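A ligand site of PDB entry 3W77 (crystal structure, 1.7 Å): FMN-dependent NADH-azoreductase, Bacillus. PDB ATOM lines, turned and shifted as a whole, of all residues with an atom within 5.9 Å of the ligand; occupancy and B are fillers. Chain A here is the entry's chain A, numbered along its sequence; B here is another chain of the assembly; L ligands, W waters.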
ATOM      1  N   ASN A  10      -2.794 -18.729  21.382  1.00  0.00           N
ATOM      2  CA  ASN A  10      -1.866 -17.894  22.153  1.00  0.00           C
ATOM      3  C   ASN A  10      -2.601 -16.695  22.716  1.00  0.00           C
ATOM      4  O   ASN A  10      -3.052 -15.860  21.939  1.00  0.00           O
ATOM      5  CB  ASN A  10      -0.767 -17.375  21.233  1.00  0.00           C
ATOM      6  CG  ASN A  10       0.394 -16.734  21.992  1.00  0.00           C
ATOM      7  OD1 ASN A  10       0.272 -16.294  23.133  1.00  0.00           O
ATOM      8  ND2 ASN A  10       1.546 -16.678  21.317  1.00  0.00           N
ATOM      9  N   ARG A  12      -1.277 -14.333  24.751  1.00  0.00           N
ATOM     10  CA  ARG A  12      -0.416 -13.153  24.928  1.00  0.00           C
ATOM     11  C   ARG A  12      -0.921 -12.011  24.041  1.00  0.00           C
ATOM     12  O   ARG A  12      -1.395 -12.259  22.951  1.00  0.00           O
ATOM     13  CB  ARG A  12       1.040 -13.463  24.570  1.00  0.00           C
ATOM     14  CG  ARG A  12       1.619 -14.613  25.401  1.00  0.00           C
ATOM     15  CD  ARG A  12       3.066 -14.929  25.053  1.00  0.00           C
ATOM     16  NE  ARG A  12       3.977 -13.852  25.520  1.00  0.00           N
ATOM     17  CZ  ARG A  12       5.227 -13.727  25.106  1.00  0.00           C
ATOM     18  NH1 ARG A  12       5.696 -14.535  24.146  1.00  0.00           N
ATOM     19  NH2 ARG A  12       5.997 -12.742  25.602  1.00  0.00           N
ATOM     20  N   GLN A  16       3.098  -8.187  22.280  1.00  0.00           N
ATOM     21  CA  GLN A  16       4.207  -8.933  22.913  1.00  0.00           C
ATOM     22  C   GLN A  16       4.509 -10.295  22.246  1.00  0.00           C
ATOM     23  O   GLN A  16       5.459 -11.008  22.642  1.00  0.00           O
ATOM     24  CB  GLN A  16       3.936  -9.131  24.406  1.00  0.00           C
ATOM     25  CG  GLN A  16       3.696  -7.829  25.170  1.00  0.00           C
ATOM     26  CD  GLN A  16       3.186  -8.018  26.598  1.00  0.00           C
ATOM     27  OE1 GLN A  16       3.099  -7.033  27.350  1.00  0.00           O
ATOM     28  NE2 GLN A  16       2.851  -9.244  26.974  1.00  0.00           N
ATOM     29  N   ALA A  17       3.688 -10.678  21.273  1.00  0.00           N
ATOM     30  CA  ALA A  17       3.772 -12.033  20.674  1.00  0.00           C
ATOM     31  C   ALA A  17       3.765 -12.075  19.144  1.00  0.00           C
ATOM     32  O   ALA A  17       2.746 -11.762  18.485  1.00  0.00           O
ATOM     33  CB  ALA A  17       2.639 -12.916  21.212  1.00  0.00           C
ATOM     34  N   VAL A  18       4.875 -12.512  18.558  1.00  0.00           N
ATOM     35  CA  VAL A  18       4.968 -12.575  17.101  1.00  0.00           C
ATOM     36  C   VAL A  18       3.908 -13.458  16.457  1.00  0.00           C
ATOM     37  O   VAL A  18       3.345 -13.099  15.421  1.00  0.00           O
ATOM     38  CB  VAL A  18       6.399 -12.985  16.623  1.00  0.00           C
ATOM     39  CG1 VAL A  18       6.470 -13.111  15.109  1.00  0.00           C
ATOM     40  CG2 VAL A  18       7.426 -11.971  17.138  1.00  0.00           C
ATOM     41  N   SER A  19       3.620 -14.624  17.060  1.00  0.00           N
ATOM     42  CA  SER A  19       2.579 -15.463  16.478  1.00  0.00           C
ATOM     43  C   SER A  19       1.204 -14.817  16.487  1.00  0.00           C
ATOM     44  O   SER A  19       0.398 -15.089  15.588  1.00  0.00           O
ATOM     45  CB  SER A  19       2.541 -16.870  17.110  1.00  0.00           C
ATOM     46  OG  SER A  19       2.154 -16.798  18.458  1.00  0.00           O
ATOM     47  N   VAL A  20       0.923 -13.983  17.487  1.00  0.00           N
ATOM     48  CA  VAL A  20      -0.370 -13.272  17.525  1.00  0.00           C
ATOM     49  C   VAL A  20      -0.416 -12.163  16.442  1.00  0.00           C
ATOM     50  O   VAL A  20      -1.400 -12.037  15.737  1.00  0.00           O
ATOM     51  CB  VAL A  20      -0.678 -12.742  18.917  1.00  0.00           C
ATOM     52  CG1 VAL A  20      -1.968 -11.950  18.904  1.00  0.00           C
ATOM     53  CG2 VAL A  20      -0.826 -13.930  19.871  1.00  0.00           C
ATOM     54  N   PHE A  97      -0.157 -20.393  15.821  1.00  0.00           N
ATOM     55  CA  PHE A  97       0.470 -20.896  17.041  1.00  0.00           C
ATOM     56  C   PHE A  97       1.954 -20.572  17.134  1.00  0.00           C
ATOM     57  O   PHE A  97       2.645 -20.512  16.122  1.00  0.00           O
ATOM     58  CB  PHE A  97       0.297 -22.451  17.110  1.00  0.00           C
ATOM     59  CG  PHE A  97       0.773 -23.193  15.878  1.00  0.00           C
ATOM     60  CD1 PHE A  97      -0.082 -23.331  14.768  1.00  0.00           C
ATOM     61  CD2 PHE A  97       2.075 -23.750  15.793  1.00  0.00           C
ATOM     62  CE1 PHE A  97       0.326 -23.989  13.607  1.00  0.00           C
ATOM     63  CE2 PHE A  97       2.481 -24.418  14.635  1.00  0.00           C
ATOM     64  CZ  PHE A  97       1.607 -24.541  13.528  1.00  0.00           C
ATOM     65  N   PRO A  98       2.453 -20.382  18.342  1.00  0.00           N
ATOM     66  CA  PRO A  98       3.905 -20.278  18.535  1.00  0.00           C
ATOM     67  C   PRO A  98       4.562 -21.650  18.636  1.00  0.00           C
ATOM     68  O   PRO A  98       3.880 -22.669  18.815  1.00  0.00           O
ATOM     69  CB  PRO A  98       3.998 -19.575  19.882  1.00  0.00           C
ATOM     70  CG  PRO A  98       2.821 -20.096  20.655  1.00  0.00           C
ATOM     71  CD  PRO A  98       1.706 -20.178  19.607  1.00  0.00           C
ATOM     72  N   LEU A  99       5.904 -21.667  18.516  1.00  0.00           N
ATOM     73  CA  LEU A  99       6.710 -22.786  19.021  1.00  0.00           C
ATOM     74  C   LEU A  99       7.130 -22.439  20.457  1.00  0.00           C
ATOM     75  O   LEU A  99       7.794 -21.415  20.694  1.00  0.00           O
ATOM     76  CB  LEU A  99       7.904 -23.036  18.082  1.00  0.00           C
ATOM     77  CG  LEU A  99       8.836 -24.202  18.499  1.00  0.00           C
ATOM     78  CD1 LEU A  99       9.476 -24.807  17.227  1.00  0.00           C
ATOM     79  CD2 LEU A  99       9.916 -23.743  19.472  1.00  0.00           C
ATOM     80  N   TRP A 100       6.655 -23.234  21.429  1.00  0.00           N
ATOM     81  CA  TRP A 100       7.034 -23.130  22.825  1.00  0.00           C
ATOM     82  C   TRP A 100       7.579 -24.455  23.233  1.00  0.00           C
ATOM     83  O   TRP A 100       6.886 -25.497  23.067  1.00  0.00           O
ATOM     84  CB  TRP A 100       5.823 -22.801  23.692  1.00  0.00           C
ATOM     85  CG  TRP A 100       5.216 -21.406  23.557  1.00  0.00           C
ATOM     86  CD1 TRP A 100       5.773 -20.251  22.991  1.00  0.00           C
ATOM     87  CD2 TRP A 100       3.920 -20.968  24.125  1.00  0.00           C
ATOM     88  NE1 TRP A 100       4.904 -19.170  23.151  1.00  0.00           N
ATOM     89  CE2 TRP A 100       3.775 -19.553  23.802  1.00  0.00           C
ATOM     90  CE3 TRP A 100       2.898 -21.626  24.804  1.00  0.00           C
ATOM     91  CZ2 TRP A 100       2.629 -18.829  24.167  1.00  0.00           C
ATOM     92  CZ3 TRP A 100       1.754 -20.893  25.166  1.00  0.00           C
ATOM     93  CH2 TRP A 100       1.627 -19.533  24.843  1.00  0.00           C
ATOM     94  N   ASN A 101       8.793 -24.476  23.783  1.00  0.00           N
ATOM     95  CA  ASN A 101       9.411 -25.738  24.243  1.00  0.00           C
ATOM     96  C   ASN A 101       9.376 -26.799  23.142  1.00  0.00           C
ATOM     97  O   ASN A 101       8.935 -27.907  23.362  1.00  0.00           O
ATOM     98  CB  ASN A 101       8.718 -26.231  25.534  1.00  0.00           C
ATOM     99  CG  ASN A 101       8.693 -25.162  26.580  1.00  0.00           C
ATOM    100  OD1 ASN A 101       9.670 -24.426  26.749  1.00  0.00           O
ATOM    101  ND2 ASN A 101       7.569 -25.045  27.299  1.00  0.00           N
ATOM    102  N   LEU A 102       9.859 -26.396  21.958  1.00  0.00           N
ATOM    103  CA  LEU A 102      10.007 -27.273  20.770  1.00  0.00           C
ATOM    104  C   LEU A 102       8.711 -27.599  20.073  1.00  0.00           C
ATOM    105  O   LEU A 102       8.746 -28.149  18.967  1.00  0.00           O
ATOM    106  CB  LEU A 102      10.772 -28.588  21.135  1.00  0.00           C
ATOM    107  CG  LEU A 102      12.170 -28.412  21.733  1.00  0.00           C
ATOM    108  CD1 LEU A 102      12.725 -29.834  21.932  1.00  0.00           C
ATOM    109  CD2 LEU A 102      13.049 -27.587  20.818  1.00  0.00           C
ATOM    110  N   THR A 103       7.560 -27.264  20.677  1.00  0.00           N
ATOM    111  CA  THR A 103       6.299 -27.793  20.115  1.00  0.00           C
ATOM    112  C   THR A 103       5.163 -26.771  20.133  1.00  0.00           C
ATOM    113  O   THR A 103       5.397 -25.592  20.322  1.00  0.00           O
ATOM    114  CB  THR A 103       5.915 -29.149  20.808  1.00  0.00           C
ATOM    115  OG1 THR A 103       4.870 -29.814  20.080  1.00  0.00           O
ATOM    116  CG2 THR A 103       5.528 -28.946  22.298  1.00  0.00           C
ATOM    117  N   ALA A 143       5.295 -18.813  14.580  1.00  0.00           N
ATOM    118  CA  ALA A 143       6.490 -18.013  14.882  1.00  0.00           C
ATOM    119  C   ALA A 143       7.364 -18.796  15.849  1.00  0.00           C
ATOM    120  O   ALA A 143       6.849 -19.474  16.754  1.00  0.00           O
ATOM    121  CB  ALA A 143       6.089 -16.691  15.521  1.00  0.00           C
ATOM    122  N   ARG A 144       8.687 -18.651  15.694  1.00  0.00           N
ATOM    123  CA  ARG A 144       9.634 -19.383  16.548  1.00  0.00           C
ATOM    124  C   ARG A 144      10.900 -18.561  16.699  1.00  0.00           C
ATOM    125  O   ARG A 144      11.395 -17.984  15.711  1.00  0.00           O
ATOM    126  CB  ARG A 144       9.904 -20.800  16.012  1.00  0.00           C
ATOM    127  CG  ARG A 144      10.281 -20.888  14.550  1.00  0.00           C
ATOM    128  CD  ARG A 144      10.043 -22.292  14.010  1.00  0.00           C
ATOM    129  NE  ARG A 144      10.625 -22.471  12.678  1.00  0.00           N
ATOM    130  CZ  ARG A 144      10.253 -23.409  11.803  1.00  0.00           C
ATOM    131  NH1 ARG A 144       9.255 -24.245  12.047  1.00  0.00           N
ATOM    132  NH2 ARG A 144      10.865 -23.483  10.657  1.00  0.00           N
ATOM    133  N   GLY A 145      11.395 -18.513  17.922  1.00  0.00           N
ATOM    134  CA  GLY A 145      12.479 -17.589  18.292  1.00  0.00           C
ATOM    135  C   GLY A 145      13.756 -17.875  17.524  1.00  0.00           C
ATOM    136  O   GLY A 145      14.432 -16.963  17.001  1.00  0.00           O
ATOM    137  N   GLY A 146      14.085 -19.162  17.459  1.00  0.00           N
ATOM    138  CA  GLY A 146      15.277 -19.590  16.727  1.00  0.00           C
ATOM    139  C   GLY A 146      14.942 -20.062  15.317  1.00  0.00           C
ATOM    140  O   GLY A 146      13.788 -20.207  14.942  1.00  0.00           O
ATOM    141  N   VAL A 147      15.982 -20.322  14.509  1.00  0.00           N
ATOM    142  CA  VAL A 147      15.785 -20.912  13.198  1.00  0.00           C
ATOM    143  C   VAL A 147      15.705 -22.445  13.343  1.00  0.00           C
ATOM    144  O   VAL A 147      16.594 -23.060  13.953  1.00  0.00           O
ATOM    145  CB  VAL A 147      16.958 -20.548  12.261  1.00  0.00           C
ATOM    146  CG1 VAL A 147      16.900 -21.358  10.971  1.00  0.00           C
ATOM    147  CG2 VAL A 147      16.919 -19.061  11.928  1.00  0.00           C
ATOM    148  N   TYR A 148      14.633 -23.037  12.799  1.00  0.00           N
ATOM    149  CA  TYR A 148      14.429 -24.473  12.779  1.00  0.00           C
ATOM    150  C   TYR A 148      14.366 -25.109  11.386  1.00  0.00           C
ATOM    151  O   TYR A 148      14.204 -26.349  11.258  1.00  0.00           O
ATOM    152  CB  TYR A 148      13.154 -24.855  13.566  1.00  0.00           C
ATOM    153  CG  TYR A 148      13.345 -24.716  15.081  1.00  0.00           C
ATOM    154  CD1 TYR A 148      13.202 -23.477  15.716  1.00  0.00           C
ATOM    155  CD2 TYR A 148      13.656 -25.849  15.860  1.00  0.00           C
ATOM    156  CE1 TYR A 148      13.374 -23.368  17.100  1.00  0.00           C
ATOM    157  CE2 TYR A 148      13.842 -25.746  17.231  1.00  0.00           C
ATOM    158  CZ  TYR A 148      13.702 -24.500  17.850  1.00  0.00           C
ATOM    159  OH  TYR A 148      13.898 -24.422  19.213  1.00  0.00           O
ATOM    160  N   HIS A 183      13.926 -14.480  14.863  1.00  0.00           N
ATOM    161  CA  HIS A 183      13.936 -13.096  15.442  1.00  0.00           C
ATOM    162  C   HIS A 183      14.563 -12.967  16.835  1.00  0.00           C
ATOM    163  O   HIS A 183      15.100 -11.893  17.173  1.00  0.00           O
ATOM    164  CB  HIS A 183      12.544 -12.480  15.400  1.00  0.00           C
ATOM    165  CG  HIS A 183      11.492 -13.383  15.959  1.00  0.00           C
ATOM    166  ND1 HIS A 183      11.050 -13.292  17.221  1.00  0.00           N
ATOM    167  CD2 HIS A 183      10.863 -14.483  15.407  1.00  0.00           C
ATOM    168  CE1 HIS A 183      10.153 -14.285  17.463  1.00  0.00           C
ATOM    169  NE2 HIS A 183      10.030 -14.995  16.351  1.00  0.00           N
ATOM    170  N   ASN A 184      14.561 -14.028  17.656  1.00  0.00           N
ATOM    171  CA  ASN A 184      15.290 -13.977  18.947  1.00  0.00           C
ATOM    172  C   ASN A 184      16.759 -14.382  18.804  1.00  0.00           C
ATOM    173  O   ASN A 184      17.641 -13.867  19.518  1.00  0.00           O
ATOM    174  CB  ASN A 184      14.618 -14.829  20.040  1.00  0.00           C
ATOM    175  CG  ASN A 184      13.261 -14.304  20.452  1.00  0.00           C
ATOM    176  OD1 ASN A 184      12.957 -13.103  20.321  1.00  0.00           O
ATOM    177  ND2 ASN A 184      12.436 -15.190  21.004  1.00  0.00           N
ATOM    178  N   VAL B  52      -0.456 -23.744  30.269  1.00  0.00           N
ATOM    179  CA  VAL B  52       0.455 -22.592  30.250  1.00  0.00           C
ATOM    180  C   VAL B  52      -0.011 -21.569  29.212  1.00  0.00           C
ATOM    181  O   VAL B  52      -0.279 -21.891  28.072  1.00  0.00           O
ATOM    182  CB  VAL B  52       1.894 -23.073  29.907  1.00  0.00           C
ATOM    183  CG1 VAL B  52       2.826 -21.888  29.661  1.00  0.00           C
ATOM    184  CG2 VAL B  52       2.390 -23.995  30.993  1.00  0.00           C
ATOM    185  N   ILE B  57       3.449 -17.494  31.766  1.00  0.00           N
ATOM    186  CA  ILE B  57       4.651 -17.002  31.067  1.00  0.00           C
ATOM    187  C   ILE B  57       5.209 -15.710  31.700  1.00  0.00           C
ATOM    188  O   ILE B  57       6.394 -15.640  32.051  1.00  0.00           O
ATOM    189  CB  ILE B  57       4.370 -16.834  29.574  1.00  0.00           C
ATOM    190  CG1 ILE B  57       4.165 -18.241  28.962  1.00  0.00           C
ATOM    191  CG2 ILE B  57       5.498 -16.073  28.884  1.00  0.00           C
ATOM    192  CD1 ILE B  57       3.571 -18.223  27.553  1.00  0.00           C
HETATM  193  N1  LIG L   1      11.932 -20.237  20.923  1.00  0.00           N
HETATM  194  C1  LIG L   1      12.654 -21.255  20.400  1.00  0.00           C
HETATM  195  O1  LIG L   1      13.395 -21.023  19.440  1.00  0.00           O
HETATM  196  N2  LIG L   1      12.602 -22.501  20.910  1.00  0.00           N
HETATM  197  C2  LIG L   1      11.818 -22.831  21.947  1.00  0.00           C
HETATM  198  O2  LIG L   1      11.740 -24.004  22.394  1.00  0.00           O
HETATM  199  C3  LIG L   1      11.000 -21.786  22.585  1.00  0.00           C
HETATM  200  N3  LIG L   1      10.190 -22.008  23.652  1.00  0.00           N
HETATM  201  C4  LIG L   1       9.450 -21.003  24.192  1.00  0.00           C
HETATM  202  C5  LIG L   1       8.613 -21.245  25.285  1.00  0.00           C
HETATM  203  C6  LIG L   1       7.829 -20.214  25.811  1.00  0.00           C
HETATM  204  C7  LIG L   1       6.898 -20.471  26.979  1.00  0.00           C
HETATM  205  C8  LIG L   1       7.876 -18.867  25.201  1.00  0.00           C
HETATM  206  C9  LIG L   1       7.056 -17.735  25.766  1.00  0.00           C
HETATM  207  C10 LIG L   1       8.720 -18.624  24.115  1.00  0.00           C
HETATM  208  C11 LIG L   1       9.506 -19.645  23.587  1.00  0.00           C
HETATM  209  N4  LIG L   1      10.348 -19.419  22.476  1.00  0.00           N
HETATM  210  C12 LIG L   1      11.131 -20.456  21.967  1.00  0.00           C
HETATM  211  C13 LIG L   1      10.375 -18.128  21.794  1.00  0.00           C
HETATM  212  C14 LIG L   1       9.154 -18.259  20.807  1.00  0.00           C
HETATM  213  O3  LIG L   1       9.225 -19.326  19.842  1.00  0.00           O
HETATM  214  C15 LIG L   1       9.092 -17.146  19.768  1.00  0.00           C
HETATM  215  O4  LIG L   1      10.071 -16.126  19.900  1.00  0.00           O
HETATM  216  C16 LIG L   1       7.818 -16.488  19.571  1.00  0.00           C
HETATM  217  O5  LIG L   1       7.805 -15.692  20.790  1.00  0.00           O
HETATM  218  C17 LIG L   1       6.690 -17.486  19.576  1.00  0.00           C
HETATM  219  O6  LIG L   1       6.240 -16.999  20.817  1.00  0.00           O
HETATM  220  P1  LIG L   1       5.144 -15.853  20.774  1.00  0.00           P
HETATM  221  O7  LIG L   1       4.309 -16.045  21.986  1.00  0.00           O
HETATM  222  O8  LIG L   1       6.026 -14.582  20.870  1.00  0.00           O
HETATM  223  O9  LIG L   1       4.432 -15.856  19.479  1.00  0.00           O
HETATM  224  O   HOH W   1      12.663 -24.169  25.621  1.00  0.00           O
HETATM  225  O   HOH W   2      13.544 -17.664  21.571  1.00  0.00           O
HETATM  226  O   HOH W   3       7.380 -11.591  20.617  1.00  0.00           O
HETATM  227  O   HOH W   4       8.928 -14.847  23.810  1.00  0.00           O
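Water W2 bridges the side-chain amide nitrogen (ND2) of Asn 184 and a nitrogen (N1) of the ligand.
Water W3 lies within hydrogen-bond range of the backbone carbonyl oxygen (O) of Gln 16 (2.9 Å), an oxygen (O8) of the ligand (3.3 Å) and the backbone NH (N) of Val 18 (3.4 Å).
Water W4 bridges NH1 of Arg 12 (3.3 Å) and O5 of the ligand (3.3 Å).
Water W1 bridges OD1 of Asn 101 (3.2 Å) and O2 of the ligand (3.4 Å).
The side-chain hydroxyl of Ser 19 lies within hydrogen-bond range of the side-chain amide nitrogen of Asn 10.
N of Leu 99 sits at hydrogen-bond distance from O of Ala 143.
O of Gly 145 sits at hydrogen-bond distance from N of Asn 184, at 3.0 Å.
N of Arg 12 lies within hydrogen-bond range of OD1 of Asn 10.
The guanidinium group of Arg 12 is in hydrogen-bond range of the backbone carbonyl oxygen of Gln 16, 3.5 Å away.
The backbone carbonyl oxygen of Gly 145 is in hydrogen-bond range of the backbone NH of His 183.
NE2 of His 183 is in hydrogen-bond range of O of Arg 144.
N of Ser 19 lies within hydrogen-bond range of O9 of the ligand, at 2.8 Å.
The side-chain hydroxyl (OG) of Ser 19 lies within hydrogen-bond range of an oxygen (O9) of the ligand (2.7 Å).
O of Leu 99 sits at hydrogen-bond distance from O3 of the ligand, at 2.7 Å.
O4 of the ligand is in hydrogen-bond range of ND2 of Asn 184 (2.8 Å).
N of Gly 146 is in hydrogen-bond range of O1 of the ligand.
N of Asn 101 sits at hydrogen-bond distance from N3 of the ligand (2.8 Å).
The side-chain hydroxyl of Tyr 148 sits at hydrogen-bond distance from a nitrogen (N2) of the ligand (2.9 Å).
An oxygen (O7) of the ligand lies within hydrogen-bond range of the side-chain amide nitrogen (ND2) of Asn 10, 2.9 Å away.
The guanidinium group (NH1) of Arg 12 is in salt-bridge range of an oxygen (O7) of the ligand.
The backbone NH (N) of Gly 145 is in hydrogen-bond range of an oxygen (O3) of the ligand (3.0 Å).
The backbone NH (N) of Leu 102 sits at hydrogen-bond distance from an oxygen (O2) of the ligand, at 3.1 Å.
The backbone NH (N) of Val 18 is in hydrogen-bond range of an oxygen (O8) of the ligand (3.3 Å).
An oxygen (O7) of the ligand is in hydrogen-bond range of the indole nitrogen (NE1) of Trp 100, 3.4 Å away.
Residues that only touch the ligand: His 183 (3.1 Å), Arg 144 (3.3 Å), Ala 17 (3.4 Å), Pro 98 (3.4 Å), Ala 143 (3.5 Å) and Ile 57 of chain B (3.9 Å).
Hydrophobic or aromatic side chains that line the ligand: Ala 17, Pro 98, Leu 99, Trp 100, Tyr 148, His 183 and Ile 57 of chain B.
Of the 24 residues printed, 18 come within 4 Å of the ligand.
The nearest printed residue that does not touch the ligand is Gln 16 (4.03 Å).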
